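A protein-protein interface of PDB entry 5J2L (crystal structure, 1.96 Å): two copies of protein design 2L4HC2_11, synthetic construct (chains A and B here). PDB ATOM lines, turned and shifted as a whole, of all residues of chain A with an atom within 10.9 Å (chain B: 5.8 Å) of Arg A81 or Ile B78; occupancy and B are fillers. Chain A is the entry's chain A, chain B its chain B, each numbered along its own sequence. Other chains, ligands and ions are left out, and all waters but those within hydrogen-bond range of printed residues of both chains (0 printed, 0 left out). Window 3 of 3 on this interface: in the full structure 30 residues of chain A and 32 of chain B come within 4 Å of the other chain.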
ATOM      1  N   SER A   6     -14.365  19.008   9.007  1.00  0.00           N
ATOM      2  CA  SER A   6     -14.113  19.434   7.631  1.00  0.00           C
ATOM      3  C   SER A   6     -13.637  20.864   7.635  1.00  0.00           C
ATOM      4  O   SER A   6     -13.047  21.339   6.658  1.00  0.00           O
ATOM      5  CB  SER A   6     -15.363  19.376   6.805  1.00  0.00           C
ATOM      6  OG  SER A   6     -16.249  20.372   7.245  1.00  0.00           O
ATOM      7  N   GLU A   7     -13.965  21.558   8.722  1.00  0.00           N
ATOM      8  CA  GLU A   7     -13.617  22.954   8.873  1.00  0.00           C
ATOM      9  C   GLU A   7     -12.112  23.111   8.836  1.00  0.00           C
ATOM     10  O   GLU A   7     -11.612  24.158   8.437  1.00  0.00           O
ATOM     11  CB  GLU A   7     -14.211  23.506  10.164  1.00  0.00           C
ATOM     12  CG  GLU A   7     -15.738  23.492  10.208  1.00  0.00           C
ATOM     13  CD  GLU A   7     -16.286  22.132  10.590  1.00  0.00           C
ATOM     14  OE1 GLU A   7     -15.897  21.149   9.985  1.00  0.00           O
ATOM     15  OE2 GLU A   7     -17.073  22.077  11.512  1.00  0.00           O
ATOM     16  N   ASP A   8     -11.391  22.056   9.229  1.00  0.00           N
ATOM     17  CA  ASP A   8      -9.939  22.091   9.215  1.00  0.00           C
ATOM     18  C   ASP A   8      -9.478  22.201   7.757  1.00  0.00           C
ATOM     19  O   ASP A   8      -8.544  22.941   7.452  1.00  0.00           O
ATOM     20  CB  ASP A   8      -9.334  20.867   9.923  1.00  0.00           C
ATOM     21  CG  ASP A   8      -7.828  20.996  10.202  1.00  0.00           C
ATOM     22  OD1 ASP A   8      -7.454  21.881  10.935  1.00  0.00           O
ATOM     23  OD2 ASP A   8      -7.065  20.202   9.705  1.00  0.00           O
ATOM     24  N   TYR A   9     -10.158  21.476   6.865  1.00  0.00           N
ATOM     25  CA  TYR A   9      -9.841  21.505   5.441  1.00  0.00           C
ATOM     26  C   TYR A   9     -10.070  22.916   4.914  1.00  0.00           C
ATOM     27  O   TYR A   9      -9.205  23.487   4.248  1.00  0.00           O
ATOM     28  CB  TYR A   9     -10.698  20.498   4.667  1.00  0.00           C
ATOM     29  CG  TYR A   9     -10.410  20.397   3.173  1.00  0.00           C
ATOM     30  CD1 TYR A   9      -9.437  19.515   2.715  1.00  0.00           C
ATOM     31  CD2 TYR A   9     -11.116  21.173   2.260  1.00  0.00           C
ATOM     32  CE1 TYR A   9      -9.188  19.394   1.354  1.00  0.00           C
ATOM     33  CE2 TYR A   9     -10.866  21.063   0.903  1.00  0.00           C
ATOM     34  CZ  TYR A   9      -9.911  20.174   0.444  1.00  0.00           C
ATOM     35  OH  TYR A   9      -9.669  20.052  -0.913  1.00  0.00           O
ATOM     36  N   LYS A  10     -11.239  23.465   5.242  1.00  0.00           N
ATOM     37  CA  LYS A  10     -11.632  24.789   4.786  1.00  0.00           C
ATOM     38  C   LYS A  10     -10.781  25.908   5.354  1.00  0.00           C
ATOM     39  O   LYS A  10     -10.551  26.914   4.682  1.00  0.00           O
ATOM     40  CB  LYS A  10     -13.098  25.031   5.105  1.00  0.00           C
ATOM     41  CG  LYS A  10     -14.029  24.287   4.190  1.00  0.00           C
ATOM     42  CD  LYS A  10     -13.926  24.921   2.817  1.00  0.00           C
ATOM     43  CE  LYS A  10     -14.897  24.338   1.813  1.00  0.00           C
ATOM     44  NZ  LYS A  10     -14.867  25.122   0.556  1.00  0.00           N
ATOM     45  N   LEU A  11     -10.315  25.734   6.579  1.00  0.00           N
ATOM     46  CA  LEU A  11      -9.517  26.758   7.217  1.00  0.00           C
ATOM     47  C   LEU A  11      -8.156  26.790   6.516  1.00  0.00           C
ATOM     48  O   LEU A  11      -7.590  27.863   6.286  1.00  0.00           O
ATOM     49  CB  LEU A  11      -9.378  26.479   8.728  1.00  0.00           C
ATOM     50  CG  LEU A  11      -8.761  27.609   9.571  1.00  0.00           C
ATOM     51  CD1 LEU A  11      -9.660  28.842   9.460  1.00  0.00           C
ATOM     52  CD2 LEU A  11      -8.627  27.171  11.023  1.00  0.00           C
ATOM     53  N   ARG A  12      -7.633  25.603   6.187  1.00  0.00           N
ATOM     54  CA  ARG A  12      -6.351  25.488   5.507  1.00  0.00           C
ATOM     55  C   ARG A  12      -6.459  26.136   4.129  1.00  0.00           C
ATOM     56  O   ARG A  12      -5.541  26.827   3.684  1.00  0.00           O
ATOM     57  CB  ARG A  12      -5.932  24.019   5.419  1.00  0.00           C
ATOM     58  CG  ARG A  12      -5.615  23.427   6.784  1.00  0.00           C
ATOM     59  CD  ARG A  12      -5.189  21.999   6.749  1.00  0.00           C
ATOM     60  NE  ARG A  12      -5.153  21.455   8.104  1.00  0.00           N
ATOM     61  CZ  ARG A  12      -4.155  21.603   8.999  1.00  0.00           C
ATOM     62  NH1 ARG A  12      -3.054  22.266   8.702  1.00  0.00           N
ATOM     63  NH2 ARG A  12      -4.324  21.064  10.193  1.00  0.00           N
ATOM     64  N   GLU A  13      -7.599  25.935   3.476  1.00  0.00           N
ATOM     65  CA  GLU A  13      -7.867  26.555   2.186  1.00  0.00           C
ATOM     66  C   GLU A  13      -7.873  28.081   2.321  1.00  0.00           C
ATOM     67  O   GLU A  13      -7.225  28.777   1.544  1.00  0.00           O
ATOM     68  CB  GLU A  13      -9.174  26.017   1.593  1.00  0.00           C
ATOM     69  CG  GLU A  13      -9.505  26.561   0.202  1.00  0.00           C
ATOM     70  CD  GLU A  13     -10.657  25.867  -0.471  1.00  0.00           C
ATOM     71  OE1 GLU A  13     -10.823  24.683  -0.280  1.00  0.00           O
ATOM     72  OE2 GLU A  13     -11.380  26.525  -1.178  1.00  0.00           O
ATOM     73  N   ALA A  14      -8.588  28.593   3.320  1.00  0.00           N
ATOM     74  CA  ALA A  14      -8.646  30.033   3.571  1.00  0.00           C
ATOM     75  C   ALA A  14      -7.245  30.599   3.755  1.00  0.00           C
ATOM     76  O   ALA A  14      -6.918  31.652   3.210  1.00  0.00           O
ATOM     77  CB  ALA A  14      -9.509  30.341   4.802  1.00  0.00           C
ATOM     78  N   GLN A  15      -6.420  29.902   4.531  1.00  0.00           N
ATOM     79  CA  GLN A  15      -5.059  30.346   4.777  1.00  0.00           C
ATOM     80  C   GLN A  15      -4.230  30.381   3.503  1.00  0.00           C
ATOM     81  O   GLN A  15      -3.519  31.357   3.247  1.00  0.00           O
ATOM     82  CB  GLN A  15      -4.396  29.459   5.818  1.00  0.00           C
ATOM     83  CG  GLN A  15      -2.964  29.837   6.142  1.00  0.00           C
ATOM     84  CD  GLN A  15      -2.830  31.182   6.810  1.00  0.00           C
ATOM     85  OE1 GLN A  15      -3.500  31.490   7.806  1.00  0.00           O
ATOM     86  NE2 GLN A  15      -1.935  31.999   6.270  1.00  0.00           N
ATOM     87  N   GLU A  73     -16.152  31.928   3.232  1.00  0.00           N
ATOM     88  CA  GLU A  73     -15.779  30.609   3.679  1.00  0.00           C
ATOM     89  C   GLU A  73     -15.581  30.564   5.189  1.00  0.00           C
ATOM     90  O   GLU A  73     -15.978  29.591   5.834  1.00  0.00           O
ATOM     91  CB  GLU A  73     -14.526  30.155   2.941  1.00  0.00           C
ATOM     92  CG  GLU A  73     -14.751  29.917   1.448  1.00  0.00           C
ATOM     93  CD  GLU A  73     -15.762  28.834   1.151  1.00  0.00           C
ATOM     94  OE1 GLU A  73     -15.592  27.735   1.631  1.00  0.00           O
ATOM     95  OE2 GLU A  73     -16.710  29.109   0.447  1.00  0.00           O
ATOM     96  N   LEU A  74     -14.993  31.623   5.752  1.00  0.00           N
ATOM     97  CA  LEU A  74     -14.755  31.664   7.188  1.00  0.00           C
ATOM     98  C   LEU A  74     -16.085  31.702   7.937  1.00  0.00           C
ATOM     99  O   LEU A  74     -16.215  31.090   9.001  1.00  0.00           O
ATOM    100  CB  LEU A  74     -13.879  32.863   7.561  1.00  0.00           C
ATOM    101  CG  LEU A  74     -12.432  32.817   7.062  1.00  0.00           C
ATOM    102  CD1 LEU A  74     -11.746  34.135   7.413  1.00  0.00           C
ATOM    103  CD2 LEU A  74     -11.705  31.637   7.668  1.00  0.00           C
ATOM    104  N   GLU A  75     -17.074  32.398   7.373  1.00  0.00           N
ATOM    105  CA  GLU A  75     -18.399  32.459   7.983  1.00  0.00           C
ATOM    106  C   GLU A  75     -19.055  31.091   7.967  1.00  0.00           C
ATOM    107  O   GLU A  75     -19.746  30.722   8.915  1.00  0.00           O
ATOM    108  CB  GLU A  75     -19.313  33.479   7.296  1.00  0.00           C
ATOM    109  CG  GLU A  75     -18.965  34.944   7.530  1.00  0.00           C
ATOM    110  CD  GLU A  75     -19.923  35.870   6.816  1.00  0.00           C
ATOM    111  OE1 GLU A  75     -20.116  35.696   5.637  1.00  0.00           O
ATOM    112  OE2 GLU A  75     -20.506  36.720   7.458  1.00  0.00           O
ATOM    113  N   LYS A  76     -18.836  30.338   6.894  1.00  0.00           N
ATOM    114  CA  LYS A  76     -19.385  28.992   6.796  1.00  0.00           C
ATOM    115  C   LYS A  76     -18.800  28.136   7.898  1.00  0.00           C
ATOM    116  O   LYS A  76     -19.522  27.383   8.556  1.00  0.00           O
ATOM    117  CB  LYS A  76     -19.082  28.376   5.432  1.00  0.00           C
ATOM    118  CG  LYS A  76     -19.829  28.996   4.259  1.00  0.00           C
ATOM    119  CD  LYS A  76     -19.377  28.359   2.951  1.00  0.00           C
ATOM    120  CE  LYS A  76     -20.027  29.018   1.742  1.00  0.00           C
ATOM    121  NZ  LYS A  76     -19.487  28.465   0.467  1.00  0.00           N
ATOM    122  N   ILE A  77     -17.494  28.274   8.110  1.00  0.00           N
ATOM    123  CA  ILE A  77     -16.794  27.540   9.152  1.00  0.00           C
ATOM    124  C   ILE A  77     -17.385  27.842  10.525  1.00  0.00           C
ATOM    125  O   ILE A  77     -17.719  26.932  11.278  1.00  0.00           O
ATOM    126  CB  ILE A  77     -15.281  27.848   9.141  1.00  0.00           C
ATOM    127  CG1 ILE A  77     -14.623  27.281   7.879  1.00  0.00           C
ATOM    128  CG2 ILE A  77     -14.615  27.293  10.388  1.00  0.00           C
ATOM    129  CD1 ILE A  77     -13.216  27.787   7.653  1.00  0.00           C
ATOM    130  N   ILE A  78     -17.526  29.120  10.845  1.00  0.00           N
ATOM    131  CA  ILE A  78     -18.077  29.516  12.136  1.00  0.00           C
ATOM    132  C   ILE A  78     -19.489  28.988  12.344  1.00  0.00           C
ATOM    133  O   ILE A  78     -19.820  28.475  13.414  1.00  0.00           O
ATOM    134  CB  ILE A  78     -18.031  31.047  12.318  1.00  0.00           C
ATOM    135  CG1 ILE A  78     -16.578  31.490  12.461  1.00  0.00           C
ATOM    136  CG2 ILE A  78     -18.869  31.494  13.511  1.00  0.00           C
ATOM    137  CD1 ILE A  78     -16.395  32.982  12.384  1.00  0.00           C
ATOM    138  N   ARG A  79     -20.321  29.103  11.323  1.00  0.00           N
ATOM    139  CA  ARG A  79     -21.693  28.646  11.425  1.00  0.00           C
ATOM    140  C   ARG A  79     -21.773  27.109  11.530  1.00  0.00           C
ATOM    141  O   ARG A  79     -22.666  26.578  12.193  1.00  0.00           O
ATOM    142  CB  ARG A  79     -22.496  29.177  10.247  1.00  0.00           C
ATOM    143  CG  ARG A  79     -22.729  30.693  10.299  1.00  0.00           C
ATOM    144  CD  ARG A  79     -23.474  31.207   9.114  1.00  0.00           C
ATOM    145  NE  ARG A  79     -23.722  32.651   9.193  1.00  0.00           N
ATOM    146  CZ  ARG A  79     -24.355  33.373   8.240  1.00  0.00           C
ATOM    147  NH1 ARG A  79     -24.788  32.783   7.148  1.00  0.00           N
ATOM    148  NH2 ARG A  79     -24.552  34.671   8.391  1.00  0.00           N
ATOM    149  N   LYS A  80     -20.832  26.397  10.904  1.00  0.00           N
ATOM    150  CA  LYS A  80     -20.816  24.931  10.942  1.00  0.00           C
ATOM    151  C   LYS A  80     -20.210  24.361  12.234  1.00  0.00           C
ATOM    152  O   LYS A  80     -20.780  23.447  12.831  1.00  0.00           O
ATOM    153  CB  LYS A  80     -20.076  24.367   9.731  1.00  0.00           C
ATOM    154  CG  LYS A  80     -20.071  22.847   9.661  1.00  0.00           C
ATOM    155  CD  LYS A  80     -19.424  22.350   8.375  1.00  0.00           C
ATOM    156  CE  LYS A  80     -19.471  20.831   8.286  1.00  0.00           C
ATOM    157  NZ  LYS A  80     -18.871  20.324   7.014  1.00  0.00           N
ATOM    158  N   ARG A  81     -19.041  24.880  12.632  1.00  0.00           N
ATOM    159  CA  ARG A  81     -18.317  24.420  13.826  1.00  0.00           C
ATOM    160  C   ARG A  81     -18.852  25.090  15.091  1.00  0.00           C
ATOM    161  O   ARG A  81     -20.048  25.388  15.188  1.00  0.00           O
ATOM    162  CB  ARG A  81     -16.809  24.680  13.699  1.00  0.00           C
ATOM    163  CG  ARG A  81     -15.958  24.241  14.899  1.00  0.00           C
ATOM    164  CD  ARG A  81     -15.651  22.783  14.890  1.00  0.00           C
ATOM    165  NE  ARG A  81     -14.678  22.442  13.860  1.00  0.00           N
ATOM    166  CZ  ARG A  81     -14.340  21.184  13.509  1.00  0.00           C
ATOM    167  NH1 ARG A  81     -14.911  20.156  14.099  1.00  0.00           N
ATOM    168  NH2 ARG A  81     -13.432  20.973  12.571  1.00  0.00           N
ATOM    169  OXT ARG A  81     -18.117  25.152  16.089  1.00  0.00           O
ATOM    170  N   LEU B  11     -16.147  32.704  18.956  1.00  0.00           N
ATOM    171  CA  LEU B  11     -16.778  32.480  17.674  1.00  0.00           C
ATOM    172  C   LEU B  11     -17.711  33.646  17.363  1.00  0.00           C
ATOM    173  O   LEU B  11     -17.731  34.136  16.235  1.00  0.00           O
ATOM    174  CB  LEU B  11     -17.524  31.147  17.676  1.00  0.00           C
ATOM    175  CG  LEU B  11     -16.637  29.891  17.730  1.00  0.00           C
ATOM    176  CD1 LEU B  11     -17.512  28.666  17.972  1.00  0.00           C
ATOM    177  CD2 LEU B  11     -15.882  29.751  16.413  1.00  0.00           C
ATOM    178  N   GLU B  73      -7.178  32.634  15.305  1.00  0.00           N
ATOM    179  CA  GLU B  73      -8.038  32.333  16.434  1.00  0.00           C
ATOM    180  C   GLU B  73      -8.944  31.128  16.133  1.00  0.00           C
ATOM    181  O   GLU B  73      -9.164  30.288  17.012  1.00  0.00           O
ATOM    182  CB  GLU B  73      -8.818  33.584  16.845  1.00  0.00           C
ATOM    183  CG  GLU B  73      -7.958  34.685  17.489  1.00  0.00           C
ATOM    184  CD  GLU B  73      -7.329  34.283  18.827  1.00  0.00           C
ATOM    185  OE1 GLU B  73      -7.986  33.589  19.566  1.00  0.00           O
ATOM    186  OE2 GLU B  73      -6.216  34.690  19.127  1.00  0.00           O
ATOM    187  N   LEU B  74      -9.423  30.999  14.893  1.00  0.00           N
ATOM    188  CA  LEU B  74     -10.201  29.820  14.536  1.00  0.00           C
ATOM    189  C   LEU B  74      -9.315  28.582  14.590  1.00  0.00           C
ATOM    190  O   LEU B  74      -9.788  27.497  14.916  1.00  0.00           O
ATOM    191  CB  LEU B  74     -10.864  29.944  13.158  1.00  0.00           C
ATOM    192  CG  LEU B  74     -12.019  30.947  13.040  1.00  0.00           C
ATOM    193  CD1 LEU B  74     -12.467  31.035  11.581  1.00  0.00           C
ATOM    194  CD2 LEU B  74     -13.165  30.485  13.922  1.00  0.00           C
ATOM    195  N   GLU B  75      -8.027  28.753  14.283  1.00  0.00           N
ATOM    196  CA  GLU B  75      -7.063  27.658  14.377  1.00  0.00           C
ATOM    197  C   GLU B  75      -7.061  27.098  15.776  1.00  0.00           C
ATOM    198  O   GLU B  75      -7.122  25.887  15.971  1.00  0.00           O
ATOM    199  CB  GLU B  75      -5.641  28.109  14.024  1.00  0.00           C
ATOM    200  CG  GLU B  75      -4.595  27.011  14.219  1.00  0.00           C
ATOM    201  CD  GLU B  75      -3.162  27.461  13.978  1.00  0.00           C
ATOM    202  OE1 GLU B  75      -2.960  28.487  13.358  1.00  0.00           O
ATOM    203  OE2 GLU B  75      -2.268  26.783  14.453  1.00  0.00           O
ATOM    204  N   LYS B  76      -6.972  27.992  16.749  1.00  0.00           N
ATOM    205  CA  LYS B  76      -6.909  27.612  18.148  1.00  0.00           C
ATOM    206  C   LYS B  76      -8.166  26.838  18.549  1.00  0.00           C
ATOM    207  O   LYS B  76      -8.091  25.824  19.245  1.00  0.00           O
ATOM    208  CB  LYS B  76      -6.724  28.863  18.989  1.00  0.00           C
ATOM    209  CG  LYS B  76      -5.377  29.528  18.782  1.00  0.00           C
ATOM    210  CD  LYS B  76      -5.273  30.827  19.557  1.00  0.00           C
ATOM    211  CE  LYS B  76      -4.020  31.593  19.156  1.00  0.00           C
ATOM    212  NZ  LYS B  76      -3.945  32.930  19.805  1.00  0.00           N
ATOM    213  N   ILE B  77      -9.318  27.314  18.082  1.00  0.00           N
ATOM    214  CA  ILE B  77     -10.584  26.670  18.415  1.00  0.00           C
ATOM    215  C   ILE B  77     -10.704  25.297  17.743  1.00  0.00           C
ATOM    216  O   ILE B  77     -10.949  24.291  18.410  1.00  0.00           O
ATOM    217  CB  ILE B  77     -11.770  27.554  18.001  1.00  0.00           C
ATOM    218  CG1 ILE B  77     -11.787  28.835  18.836  1.00  0.00           C
ATOM    219  CG2 ILE B  77     -13.068  26.782  18.196  1.00  0.00           C
ATOM    220  CD1 ILE B  77     -12.742  29.892  18.309  1.00  0.00           C
ATOM    221  N   ILE B  78     -10.534  25.273  16.424  1.00  0.00           N
ATOM    222  CA  ILE B  78     -10.615  24.054  15.632  1.00  0.00           C
ATOM    223  C   ILE B  78      -9.572  23.043  16.084  1.00  0.00           C
ATOM    224  O   ILE B  78      -9.867  21.855  16.180  1.00  0.00           O
ATOM    225  CB  ILE B  78     -10.530  24.385  14.121  1.00  0.00           C
ATOM    226  CG1 ILE B  78     -11.838  25.094  13.715  1.00  0.00           C
ATOM    227  CG2 ILE B  78     -10.278  23.147  13.272  1.00  0.00           C
ATOM    228  CD1 ILE B  78     -11.813  25.706  12.333  1.00  0.00           C
ATOM    229  N   ARG B  79      -8.367  23.508  16.383  1.00  0.00           N
ATOM    230  CA  ARG B  79      -7.346  22.636  16.953  1.00  0.00           C
ATOM    231  C   ARG B  79      -7.963  21.884  18.118  1.00  0.00           C
ATOM    232  O   ARG B  79      -7.870  20.653  18.200  1.00  0.00           O
ATOM    233  CB  ARG B  79      -6.141  23.435  17.419  1.00  0.00           C
ATOM    234  CG  ARG B  79      -5.023  22.630  18.057  1.00  0.00           C
ATOM    235  CD  ARG B  79      -3.942  23.520  18.577  1.00  0.00           C
ATOM    236  NE  ARG B  79      -3.228  24.225  17.513  1.00  0.00           N
ATOM    237  CZ  ARG B  79      -2.164  23.740  16.834  1.00  0.00           C
ATOM    238  NH1 ARG B  79      -1.680  22.546  17.122  1.00  0.00           N
ATOM    239  NH2 ARG B  79      -1.604  24.469  15.875  1.00  0.00           N
ATOM    240  N   LYS B  80      -8.603  22.633  19.016  1.00  0.00           N
ATOM    241  CA  LYS B  80      -9.281  22.079  20.180  1.00  0.00           C
ATOM    242  C   LYS B  80     -10.482  21.227  19.771  1.00  0.00           C
ATOM    243  O   LYS B  80     -10.867  20.306  20.492  1.00  0.00           O
ATOM    244  CB  LYS B  80      -9.720  23.201  21.119  1.00  0.00           C
ATOM    245  CG  LYS B  80      -8.567  23.915  21.794  1.00  0.00           C
ATOM    246  CD  LYS B  80      -9.059  25.034  22.698  1.00  0.00           C
ATOM    247  CE  LYS B  80      -7.891  25.741  23.385  1.00  0.00           C
ATOM    248  NZ  LYS B  80      -8.355  26.832  24.289  1.00  0.00           N
ATOM    249  N   ARG B  81     -11.070  21.542  18.614  1.00  0.00           N
ATOM    250  CA  ARG B  81     -12.229  20.801  18.116  1.00  0.00           C
ATOM    251  C   ARG B  81     -11.828  19.878  16.950  1.00  0.00           C
ATOM    252  O   ARG B  81     -10.958  19.014  17.109  1.00  0.00           O
ATOM    253  CB  ARG B  81     -13.344  21.767  17.688  1.00  0.00           C
ATOM    254  CG  ARG B  81     -13.911  22.635  18.820  1.00  0.00           C
ATOM    255  CD  ARG B  81     -15.043  23.519  18.375  1.00  0.00           C
ATOM    256  NE  ARG B  81     -15.523  24.356  19.473  1.00  0.00           N
ATOM    257  CZ  ARG B  81     -16.654  25.100  19.486  1.00  0.00           C
ATOM    258  NH1 ARG B  81     -17.477  25.126  18.456  1.00  0.00           N
ATOM    259  NH2 ARG B  81     -16.928  25.815  20.568  1.00  0.00           N
ATOM    260  OXT ARG B  81     -12.561  19.817  15.961  1.00  0.00           O
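CB of Glu A7 touches CD1 of Ile B78, 3.9 Å away.
OD1 of Asp A8 touches CG2 of Ile B78, at 3.9 Å.
Leu A11 touches Leu B74 (CD2 to C, 3.9 Å).
N of Glu B75 touches CD2 of Leu A11, at 3.7 Å.
Leu A11 touches Ile B78.
Ile B78 touches Ile A77.
O of Leu B11 touches CG2 of Ile A78, 3.96 Å away.
CG1 of Ile A78 touches CD2 of Leu B74 (3.8 Å).
Arg A81 touches Ile B78 (NE to CG1, 3.9 Å).
Printed residues of chain B that touch a printed residue of chain A: Leu B11, Leu B74, Glu B75, Ile B78 and Arg B81.
Printed residues of chain A that touch a printed residue of chain B: Glu A7, Asp A8, Leu A11, Ile A77, Ile A78 and Arg A81.
Hydrophobic or aromatic side chains of chain A that line the printed part of chain B: Leu A11, Ile A77 and Ile A78.
Among the printed residues, 10 pairs touch across the chains.
Among the printed residues, no Asp or Glu carboxylate lies within 4 Å of a Lys or Arg side-chain nitrogen of the other chain.
OXT of Arg A81 is in salt-bridge range of NH1 of Arg B81 (2.5 Å).
The side-chain carboxylate of Glu B75 is in salt-bridge range of the guanidinium group of Arg B79 (2.8 Å).
The side-chain hydroxyl (OG) of Ser A6 sits at hydrogen-bond distance from the side-chain carboxylate (OE1) of Glu A7 (2.9 Å).
The side-chain carboxylate (OE2) of Glu A7 lies within salt-bridge range of the guanidinium group (NE) of Arg A81 (3.4 Å).
NE of Arg A12 is in salt-bridge range of OD2 of Asp A8.
Arg A81 touches just these residues of chain B: Ile B78 and Arg B81.
Leu B74 touches two residues of chain A.
No residue of chain A comes within 4 Å of Ile B77.
Of chain A, only Arg A81 comes within 4 Å of Arg B81.
Of the printed residues of chain B, Asp A8 touches Ile B78.
Of the printed residues of chain B, Glu A7 touches Ile B78.
Lys A80 touches none of the printed residues of chain B.
Glu A73 touches none of the printed residues of chain B.
The nearest residue of chain A that does not touch Ile B78 is Tyr A9 (6.6 Å).
Leu A11 touches Leu B74, but with the chains exchanged Leu A74 does not touch Leu B11 (7.5 Å).
Leu A11 touches Glu B75, but with the chains exchanged Glu A75 does not touch Leu B11 (8.3 Å).
Ile A78 touches Leu B74, but with the chains exchanged Leu A74 does not touch Ile B78 (7.5 Å).
Arg A81 touches Ile B78, but with the chains exchanged Ile A78 does not touch Arg B81 (6.5 Å).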
